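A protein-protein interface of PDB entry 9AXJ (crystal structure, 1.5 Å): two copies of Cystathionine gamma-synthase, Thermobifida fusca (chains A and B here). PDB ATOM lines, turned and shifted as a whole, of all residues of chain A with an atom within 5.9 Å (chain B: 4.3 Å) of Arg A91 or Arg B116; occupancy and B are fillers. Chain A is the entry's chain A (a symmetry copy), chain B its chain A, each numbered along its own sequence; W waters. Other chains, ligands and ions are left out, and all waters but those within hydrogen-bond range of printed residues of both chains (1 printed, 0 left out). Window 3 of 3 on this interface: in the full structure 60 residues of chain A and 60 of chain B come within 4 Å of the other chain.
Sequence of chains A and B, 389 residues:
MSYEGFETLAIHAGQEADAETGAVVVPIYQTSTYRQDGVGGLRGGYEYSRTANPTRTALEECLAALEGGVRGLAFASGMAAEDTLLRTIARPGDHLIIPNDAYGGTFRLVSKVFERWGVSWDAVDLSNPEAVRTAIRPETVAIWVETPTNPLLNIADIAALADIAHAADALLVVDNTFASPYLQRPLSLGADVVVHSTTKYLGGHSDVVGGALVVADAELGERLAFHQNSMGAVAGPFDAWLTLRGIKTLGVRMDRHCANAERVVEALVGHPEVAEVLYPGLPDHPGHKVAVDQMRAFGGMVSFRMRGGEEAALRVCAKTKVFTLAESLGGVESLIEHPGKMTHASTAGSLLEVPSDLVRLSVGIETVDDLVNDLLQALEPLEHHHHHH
NH2 of Arg B116 sits at hydrogen-bond distance from O of Arg A87. NH2 of Arg B116 sits at hydrogen-bond distance from O of Thr A88, 2.9 Å away. The guanidinium group (NH2) of Arg B116 is in hydrogen-bond range of the backbone carbonyl oxygen (O) of Ala A90, 2.6 Å away. The backbone carbonyl oxygen (O) of Arg B116 is in hydrogen-bond range of the guanidinium group (NH2) of Arg A91, at 2.9 Å. The indole nitrogen (NE1) of Trp B117 is in hydrogen-bond range of the backbone carbonyl oxygen (O) of Arg A87.
The backbone NH (N) of Arg A91 lies within hydrogen-bond range of the side-chain carboxylate (OD2) of Asp A94, 2.9 Å away. ND1 of His A227 is in hydrogen-bond range of OG1 of Thr A88.
Among the printed residues, pairs that only touch across the chains: Ala A90 with Trp B117, Trp A117 with Trp B117, Pro A92 with Trp B117, Arg A91 with Trp B117, Pro A92 with Arg B116, Trp A117 with Phe B114, Val A119 with Trp B117, Leu A86 with Trp B117, Arg A87 with Phe B114, Arg A87 with Val B113 and His A227 with Val B113.
Of the printed residues of chain B, Leu A86 touches Trp B117. Printed residues of chain B within 4 Å of Thr A88: Arg B116 (2.9 Å). Of the printed residues of chain B, Arg A91 touches Arg B116 (2.9 Å) and Trp B117 (3.7 Å). Printed residues of chain B within 4 Å of Pro A92: Arg B116 (3.7 Å) and Trp B117 (3.5 Å). His A95 touches none of the printed residues of chain B. Printed residues of chain A within 4 Å of Arg B116: Arg A87, Thr A88, Ala A90, Arg A91 and Pro A92. Printed residues of chain A within 4 Å of Trp B117: Leu A86, Arg A87, Ala A90, Arg A91, Pro A92, Trp A117 and Val A119. The nearest printed residue of chain B that does not touch Arg A91 is Glu B115 (5.2 Å).
Of the 6 printed residues of chain B, 4 touch a printed residue of chain A. Hydrophobic or aromatic side chains of chain B within 4 Å of the printed part of chain A: Val B113, Phe B114 and Trp B117. Of the 14 printed residues of chain A, 9 touch a printed residue of chain B. Hydrophobic or aromatic side chains of chain A within 4 Å of the printed part of chain B: Pro A92, Trp A117, Val A119 and His A227. Among the printed residues, 16 pairs touch across the chains. Among the printed residues, no Asp or Glu carboxylate lies within 4 Å of a Lys or Arg side-chain nitrogen of the other chain.
Trp A117 touches its own counterpart, Trp B117. 2 positions are printed for both chains.
Water W1 bridges NH1 of Arg A91 (3.1 Å) and NH1 of Arg B116 (3.5 Å).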
ATOM      1  N   LEU A  86     -22.182  13.279  24.843  1.00  0.00           N
ATOM      2  CA  LEU A  86     -22.406  14.474  25.684  1.00  0.00           C
ATOM      3  C   LEU A  86     -22.420  15.746  24.847  1.00  0.00           C
ATOM      4  O   LEU A  86     -23.203  16.656  25.143  1.00  0.00           O
ATOM      5  CB  LEU A  86     -21.372  14.521  26.816  1.00  0.00           C
ATOM      6  CG  LEU A  86     -21.483  13.433  27.887  1.00  0.00           C
ATOM      7  CD1 LEU A  86     -20.336  13.561  28.896  1.00  0.00           C
ATOM      8  CD2 LEU A  86     -22.832  13.409  28.561  1.00  0.00           C
ATOM      9  N   ARG A  87     -21.602  15.826  23.784  1.00  0.00           N
ATOM     10  CA  ARG A  87     -21.608  17.030  22.912  1.00  0.00           C
ATOM     11  C   ARG A  87     -22.969  17.113  22.234  1.00  0.00           C
ATOM     12  O   ARG A  87     -23.423  18.212  21.978  1.00  0.00           O
ATOM     13  CB  ARG A  87     -20.506  17.012  21.852  1.00  0.00           C
ATOM     14  CG  ARG A  87     -20.111  18.386  21.392  1.00  0.00           C
ATOM     15  CD  ARG A  87     -19.123  18.986  22.412  1.00  0.00           C
ATOM     16  NE  ARG A  87     -17.885  18.234  22.332  1.00  0.00           N
ATOM     17  CZ  ARG A  87     -16.996  18.359  21.316  1.00  0.00           C
ATOM     18  NH1 ARG A  87     -15.926  17.574  21.391  1.00  0.00           N
ATOM     19  NH2 ARG A  87     -17.205  19.187  20.224  1.00  0.00           N
ATOM     20  N   THR A  88     -23.579  15.960  21.933  1.00  0.00           N
ATOM     21  CA  THR A  88     -24.866  15.890  21.209  1.00  0.00           C
ATOM     22  C   THR A  88     -26.001  16.293  22.157  1.00  0.00           C
ATOM     23  O   THR A  88     -26.901  17.095  21.753  1.00  0.00           O
ATOM     24  CB  THR A  88     -25.104  14.495  20.645  1.00  0.00           C
ATOM     25  OG1 THR A  88     -24.078  14.160  19.725  1.00  0.00           O
ATOM     26  CG2 THR A  88     -26.432  14.383  19.960  1.00  0.00           C
ATOM     27  N   ILE A  89     -26.072  15.714  23.360  1.00  0.00           N
ATOM     28  CA  ILE A  89     -27.308  15.809  24.189  1.00  0.00           C
ATOM     29  C   ILE A  89     -27.225  16.981  25.171  1.00  0.00           C
ATOM     30  O   ILE A  89     -28.252  17.292  25.743  1.00  0.00           O
ATOM     31  CB  ILE A  89     -27.601  14.478  24.917  1.00  0.00           C
ATOM     32  CG1 ILE A  89     -26.586  14.172  26.018  1.00  0.00           C
ATOM     33  CG2 ILE A  89     -27.767  13.356  23.912  1.00  0.00           C
ATOM     34  CD1 ILE A  89     -26.989  13.040  26.933  1.00  0.00           C
ATOM     35  N   ALA A  90     -26.061  17.592  25.399  1.00  0.00           N
ATOM     36  CA  ALA A  90     -25.878  18.677  26.379  1.00  0.00           C
ATOM     37  C   ALA A  90     -25.484  19.941  25.650  1.00  0.00           C
ATOM     38  O   ALA A  90     -25.175  19.929  24.443  1.00  0.00           O
ATOM     39  CB  ALA A  90     -24.872  18.316  27.468  1.00  0.00           C
ATOM     40  N   ARG A  91     -25.563  21.047  26.365  1.00  0.00           N
ATOM     41  CA  ARG A  91     -25.088  22.361  25.900  1.00  0.00           C
ATOM     42  C   ARG A  91     -24.787  23.124  27.192  1.00  0.00           C
ATOM     43  O   ARG A  91     -25.131  22.578  28.273  1.00  0.00           O
ATOM     44  CB  ARG A  91     -26.146  22.961  24.963  1.00  0.00           C
ATOM     45  CG  ARG A  91     -27.407  23.408  25.639  1.00  0.00           C
ATOM     46  CD  ARG A  91     -28.451  23.992  24.654  1.00  0.00           C
ATOM     47  NE  ARG A  91     -27.927  25.168  24.031  1.00  0.00           N
ATOM     48  CZ  ARG A  91     -27.926  25.406  22.735  1.00  0.00           C
ATOM     49  NH1 ARG A  91     -28.461  24.536  21.868  1.00  0.00           N
ATOM     50  NH2 ARG A  91     -27.321  26.477  22.332  1.00  0.00           N
ATOM     51  N   PRO A  92     -24.153  24.348  27.088  1.00  0.00           N
ATOM     52  CA  PRO A  92     -23.923  25.180  28.274  1.00  0.00           C
ATOM     53  C   PRO A  92     -25.246  25.412  29.023  1.00  0.00           C
ATOM     54  O   PRO A  92     -26.242  25.764  28.430  1.00  0.00           O
ATOM     55  CB  PRO A  92     -23.257  26.429  27.731  1.00  0.00           C
ATOM     56  CG  PRO A  92     -22.625  25.965  26.409  1.00  0.00           C
ATOM     57  CD  PRO A  92     -23.616  24.949  25.852  1.00  0.00           C
ATOM     58  N   GLY A  93     -25.190  25.302  30.332  1.00  0.00           N
ATOM     59  CA  GLY A  93     -26.330  25.532  31.217  1.00  0.00           C
ATOM     60  C   GLY A  93     -27.006  24.252  31.657  1.00  0.00           C
ATOM     61  O   GLY A  93     -27.847  24.326  32.583  1.00  0.00           O
ATOM     62  N   ASP A  94     -26.699  23.139  31.015  1.00  0.00           N
ATOM     63  CA  ASP A  94     -27.340  21.845  31.313  1.00  0.00           C
ATOM     64  C   ASP A  94     -26.663  21.234  32.526  1.00  0.00           C
ATOM     65  O   ASP A  94     -25.575  21.688  32.934  1.00  0.00           O
ATOM     66  CB  ASP A  94     -27.293  20.885  30.123  1.00  0.00           C
ATOM     67  CG  ASP A  94     -28.169  21.308  28.980  1.00  0.00           C
ATOM     68  OD1 ASP A  94     -29.060  22.166  29.198  1.00  0.00           O
ATOM     69  OD2 ASP A  94     -27.994  20.699  27.904  1.00  0.00           O
ATOM     70  N   HIS A  95     -27.291  20.228  33.092  1.00  0.00           N
ATOM     71  CA  HIS A  95     -26.809  19.497  34.289  1.00  0.00           C
ATOM     72  C   HIS A  95     -26.817  18.018  33.993  1.00  0.00           C
ATOM     73  O   HIS A  95     -27.738  17.517  33.284  1.00  0.00           O
ATOM     74  CB  HIS A  95     -27.693  19.843  35.480  1.00  0.00           C
ATOM     75  CG  HIS A  95     -27.419  19.073  36.713  1.00  0.00           C
ATOM     76  ND1 HIS A  95     -28.233  18.004  37.117  1.00  0.00           N
ATOM     77  CD2 HIS A  95     -26.466  19.211  37.657  1.00  0.00           C
ATOM     78  CE1 HIS A  95     -27.768  17.530  38.250  1.00  0.00           C
ATOM     79  NE2 HIS A  95     -26.710  18.260  38.632  1.00  0.00           N
ATOM     80  N   TRP A 117     -16.965  23.905  29.848  1.00  0.00           N
ATOM     81  CA  TRP A 117     -17.852  24.186  28.699  1.00  0.00           C
ATOM     82  C   TRP A 117     -19.287  24.419  29.172  1.00  0.00           C
ATOM     83  O   TRP A 117     -20.212  24.453  28.338  1.00  0.00           O
ATOM     84  CB  TRP A 117     -17.708  23.085  27.642  1.00  0.00           C
ATOM     85  CG  TRP A 117     -16.520  23.256  26.757  1.00  0.00           C
ATOM     86  CD1 TRP A 117     -15.254  22.808  26.919  1.00  0.00           C
ATOM     87  CD2 TRP A 117     -16.501  24.053  25.580  1.00  0.00           C
ATOM     88  NE1 TRP A 117     -14.450  23.230  25.893  1.00  0.00           N
ATOM     89  CE2 TRP A 117     -15.199  24.000  25.054  1.00  0.00           C
ATOM     90  CE3 TRP A 117     -17.498  24.792  24.913  1.00  0.00           C
ATOM     91  CZ2 TRP A 117     -14.840  24.699  23.911  1.00  0.00           C
ATOM     92  CZ3 TRP A 117     -17.141  25.488  23.776  1.00  0.00           C
ATOM     93  CH2 TRP A 117     -15.833  25.428  23.297  1.00  0.00           C
ATOM     94  N   GLY A 118     -19.487  24.627  30.469  1.00  0.00           N
ATOM     95  CA  GLY A 118     -20.725  25.124  31.058  1.00  0.00           C
ATOM     96  C   GLY A 118     -21.733  24.081  31.503  1.00  0.00           C
ATOM     97  O   GLY A 118     -22.864  24.510  31.819  1.00  0.00           O
ATOM     98  N   VAL A 119     -21.336  22.802  31.626  1.00  0.00           N
ATOM     99  CA  VAL A 119     -22.250  21.736  32.088  1.00  0.00           C
ATOM    100  C   VAL A 119     -22.018  21.498  33.555  1.00  0.00           C
ATOM    101  O   VAL A 119     -20.881  21.232  33.946  1.00  0.00           O
ATOM    102  CB  VAL A 119     -22.078  20.438  31.283  1.00  0.00           C
ATOM    103  CG1 VAL A 119     -23.017  19.344  31.787  1.00  0.00           C
ATOM    104  CG2 VAL A 119     -22.300  20.685  29.806  1.00  0.00           C
ATOM    105  N   HIS A 227     -22.976  14.122  14.771  1.00  0.00           N
ATOM    106  CA  HIS A 227     -21.759  14.445  15.569  1.00  0.00           C
ATOM    107  C   HIS A 227     -20.635  13.449  15.271  1.00  0.00           C
ATOM    108  O   HIS A 227     -19.448  13.828  15.296  1.00  0.00           O
ATOM    109  CB  HIS A 227     -22.093  14.618  17.033  1.00  0.00           C
ATOM    110  CG  HIS A 227     -22.905  15.834  17.295  1.00  0.00           C
ATOM    111  ND1 HIS A 227     -24.293  15.865  17.149  1.00  0.00           N
ATOM    112  CD2 HIS A 227     -22.537  17.059  17.725  1.00  0.00           C
ATOM    113  CE1 HIS A 227     -24.711  17.118  17.430  1.00  0.00           C
ATOM    114  NE2 HIS A 227     -23.685  17.830  17.823  1.00  0.00           N
ATOM    115  N   VAL B 113     -21.837  23.036  15.541  1.00  0.00           N
ATOM    116  CA  VAL B 113     -21.515  22.417  16.865  1.00  0.00           C
ATOM    117  C   VAL B 113     -20.959  23.491  17.819  1.00  0.00           C
ATOM    118  O   VAL B 113     -21.564  23.731  18.875  1.00  0.00           O
ATOM    119  CB  VAL B 113     -20.544  21.247  16.754  1.00  0.00           C
ATOM    120  CG1 VAL B 113     -20.283  20.622  18.129  1.00  0.00           C
ATOM    121  CG2 VAL B 113     -21.066  20.205  15.774  1.00  0.00           C
ATOM    122  N   PHE B 114     -19.904  24.184  17.456  1.00  0.00           N
ATOM    123  CA  PHE B 114     -19.295  25.060  18.449  1.00  0.00           C
ATOM    124  C   PHE B 114     -20.177  26.306  18.729  1.00  0.00           C
ATOM    125  O   PHE B 114     -20.173  26.837  19.810  1.00  0.00           O
ATOM    126  CB  PHE B 114     -17.876  25.417  18.061  1.00  0.00           C
ATOM    127  CG  PHE B 114     -16.876  24.375  18.505  1.00  0.00           C
ATOM    128  CD1 PHE B 114     -16.686  23.236  17.722  1.00  0.00           C
ATOM    129  CD2 PHE B 114     -16.207  24.468  19.713  1.00  0.00           C
ATOM    130  CE1 PHE B 114     -15.873  22.203  18.145  1.00  0.00           C
ATOM    131  CE2 PHE B 114     -15.332  23.453  20.106  1.00  0.00           C
ATOM    132  CZ  PHE B 114     -15.163  22.339  19.324  1.00  0.00           C
ATOM    133  N   GLU B 115     -20.936  26.765  17.761  1.00  0.00           N
ATOM    134  CA  GLU B 115     -21.838  27.940  17.993  1.00  0.00           C
ATOM    135  C   GLU B 115     -22.854  27.589  19.059  1.00  0.00           C
ATOM    136  O   GLU B 115     -23.103  28.430  19.930  1.00  0.00           O
ATOM    137  CB  GLU B 115     -22.474  28.402  16.675  1.00  0.00           C
ATOM    138  CG  GLU B 115     -23.267  29.693  16.876  1.00  0.00           C
ATOM    139  CD  GLU B 115     -24.005  30.159  15.633  1.00  0.00           C
ATOM    140  OE1 GLU B 115     -25.153  30.491  15.778  1.00  0.00           O
ATOM    141  OE2 GLU B 115     -23.438  30.133  14.545  1.00  0.00           O
ATOM    142  N   ARG B 116     -23.444  26.394  18.993  1.00  0.00           N
ATOM    143  CA  ARG B 116     -24.459  25.855  19.952  1.00  0.00           C
ATOM    144  C   ARG B 116     -23.808  25.763  21.342  1.00  0.00           C
ATOM    145  O   ARG B 116     -24.511  25.877  22.356  1.00  0.00           O
ATOM    146  CB  ARG B 116     -24.957  24.534  19.342  1.00  0.00           C
ATOM    147  CG  ARG B 116     -25.995  23.735  20.118  1.00  0.00           C
ATOM    148  CD  ARG B 116     -26.422  22.423  19.416  1.00  0.00           C
ATOM    149  NE  ARG B 116     -25.993  21.246  20.219  1.00  0.00           N
ATOM    150  CZ  ARG B 116     -26.577  20.928  21.347  1.00  0.00           C
ATOM    151  NH1 ARG B 116     -27.669  21.572  21.676  1.00  0.00           N
ATOM    152  NH2 ARG B 116     -26.180  19.907  22.066  1.00  0.00           N
ATOM    153  N   TRP B 117     -22.500  25.593  21.385  1.00  0.00           N
ATOM    154  CA  TRP B 117     -21.697  25.469  22.621  1.00  0.00           C
ATOM    155  C   TRP B 117     -21.108  26.822  23.017  1.00  0.00           C
ATOM    156  O   TRP B 117     -20.231  26.876  23.900  1.00  0.00           O
ATOM    157  CB  TRP B 117     -20.659  24.352  22.461  1.00  0.00           C
ATOM    158  CG  TRP B 117     -21.209  22.985  22.691  1.00  0.00           C
ATOM    159  CD1 TRP B 117     -21.778  22.128  21.813  1.00  0.00           C
ATOM    160  CD2 TRP B 117     -21.323  22.366  23.965  1.00  0.00           C
ATOM    161  NE1 TRP B 117     -22.199  20.988  22.445  1.00  0.00           N
ATOM    162  CE2 TRP B 117     -21.928  21.112  23.775  1.00  0.00           C
ATOM    163  CE3 TRP B 117     -20.935  22.769  25.259  1.00  0.00           C
ATOM    164  CZ2 TRP B 117     -22.207  20.263  24.836  1.00  0.00           C
ATOM    165  CZ3 TRP B 117     -21.213  21.925  26.315  1.00  0.00           C
ATOM    166  CH2 TRP B 117     -21.834  20.697  26.087  1.00  0.00           C
ATOM    167  N   GLY B 118     -21.598  27.909  22.430  1.00  0.00           N
ATOM    168  CA  GLY B 118     -21.357  29.279  22.865  1.00  0.00           C
ATOM    169  C   GLY B 118     -20.173  29.992  22.239  1.00  0.00           C
ATOM    170  O   GLY B 118     -19.853  31.085  22.757  1.00  0.00           O
HETATM  171  O   HOH W   1     -30.799  22.734  20.787  1.00  0.00           O
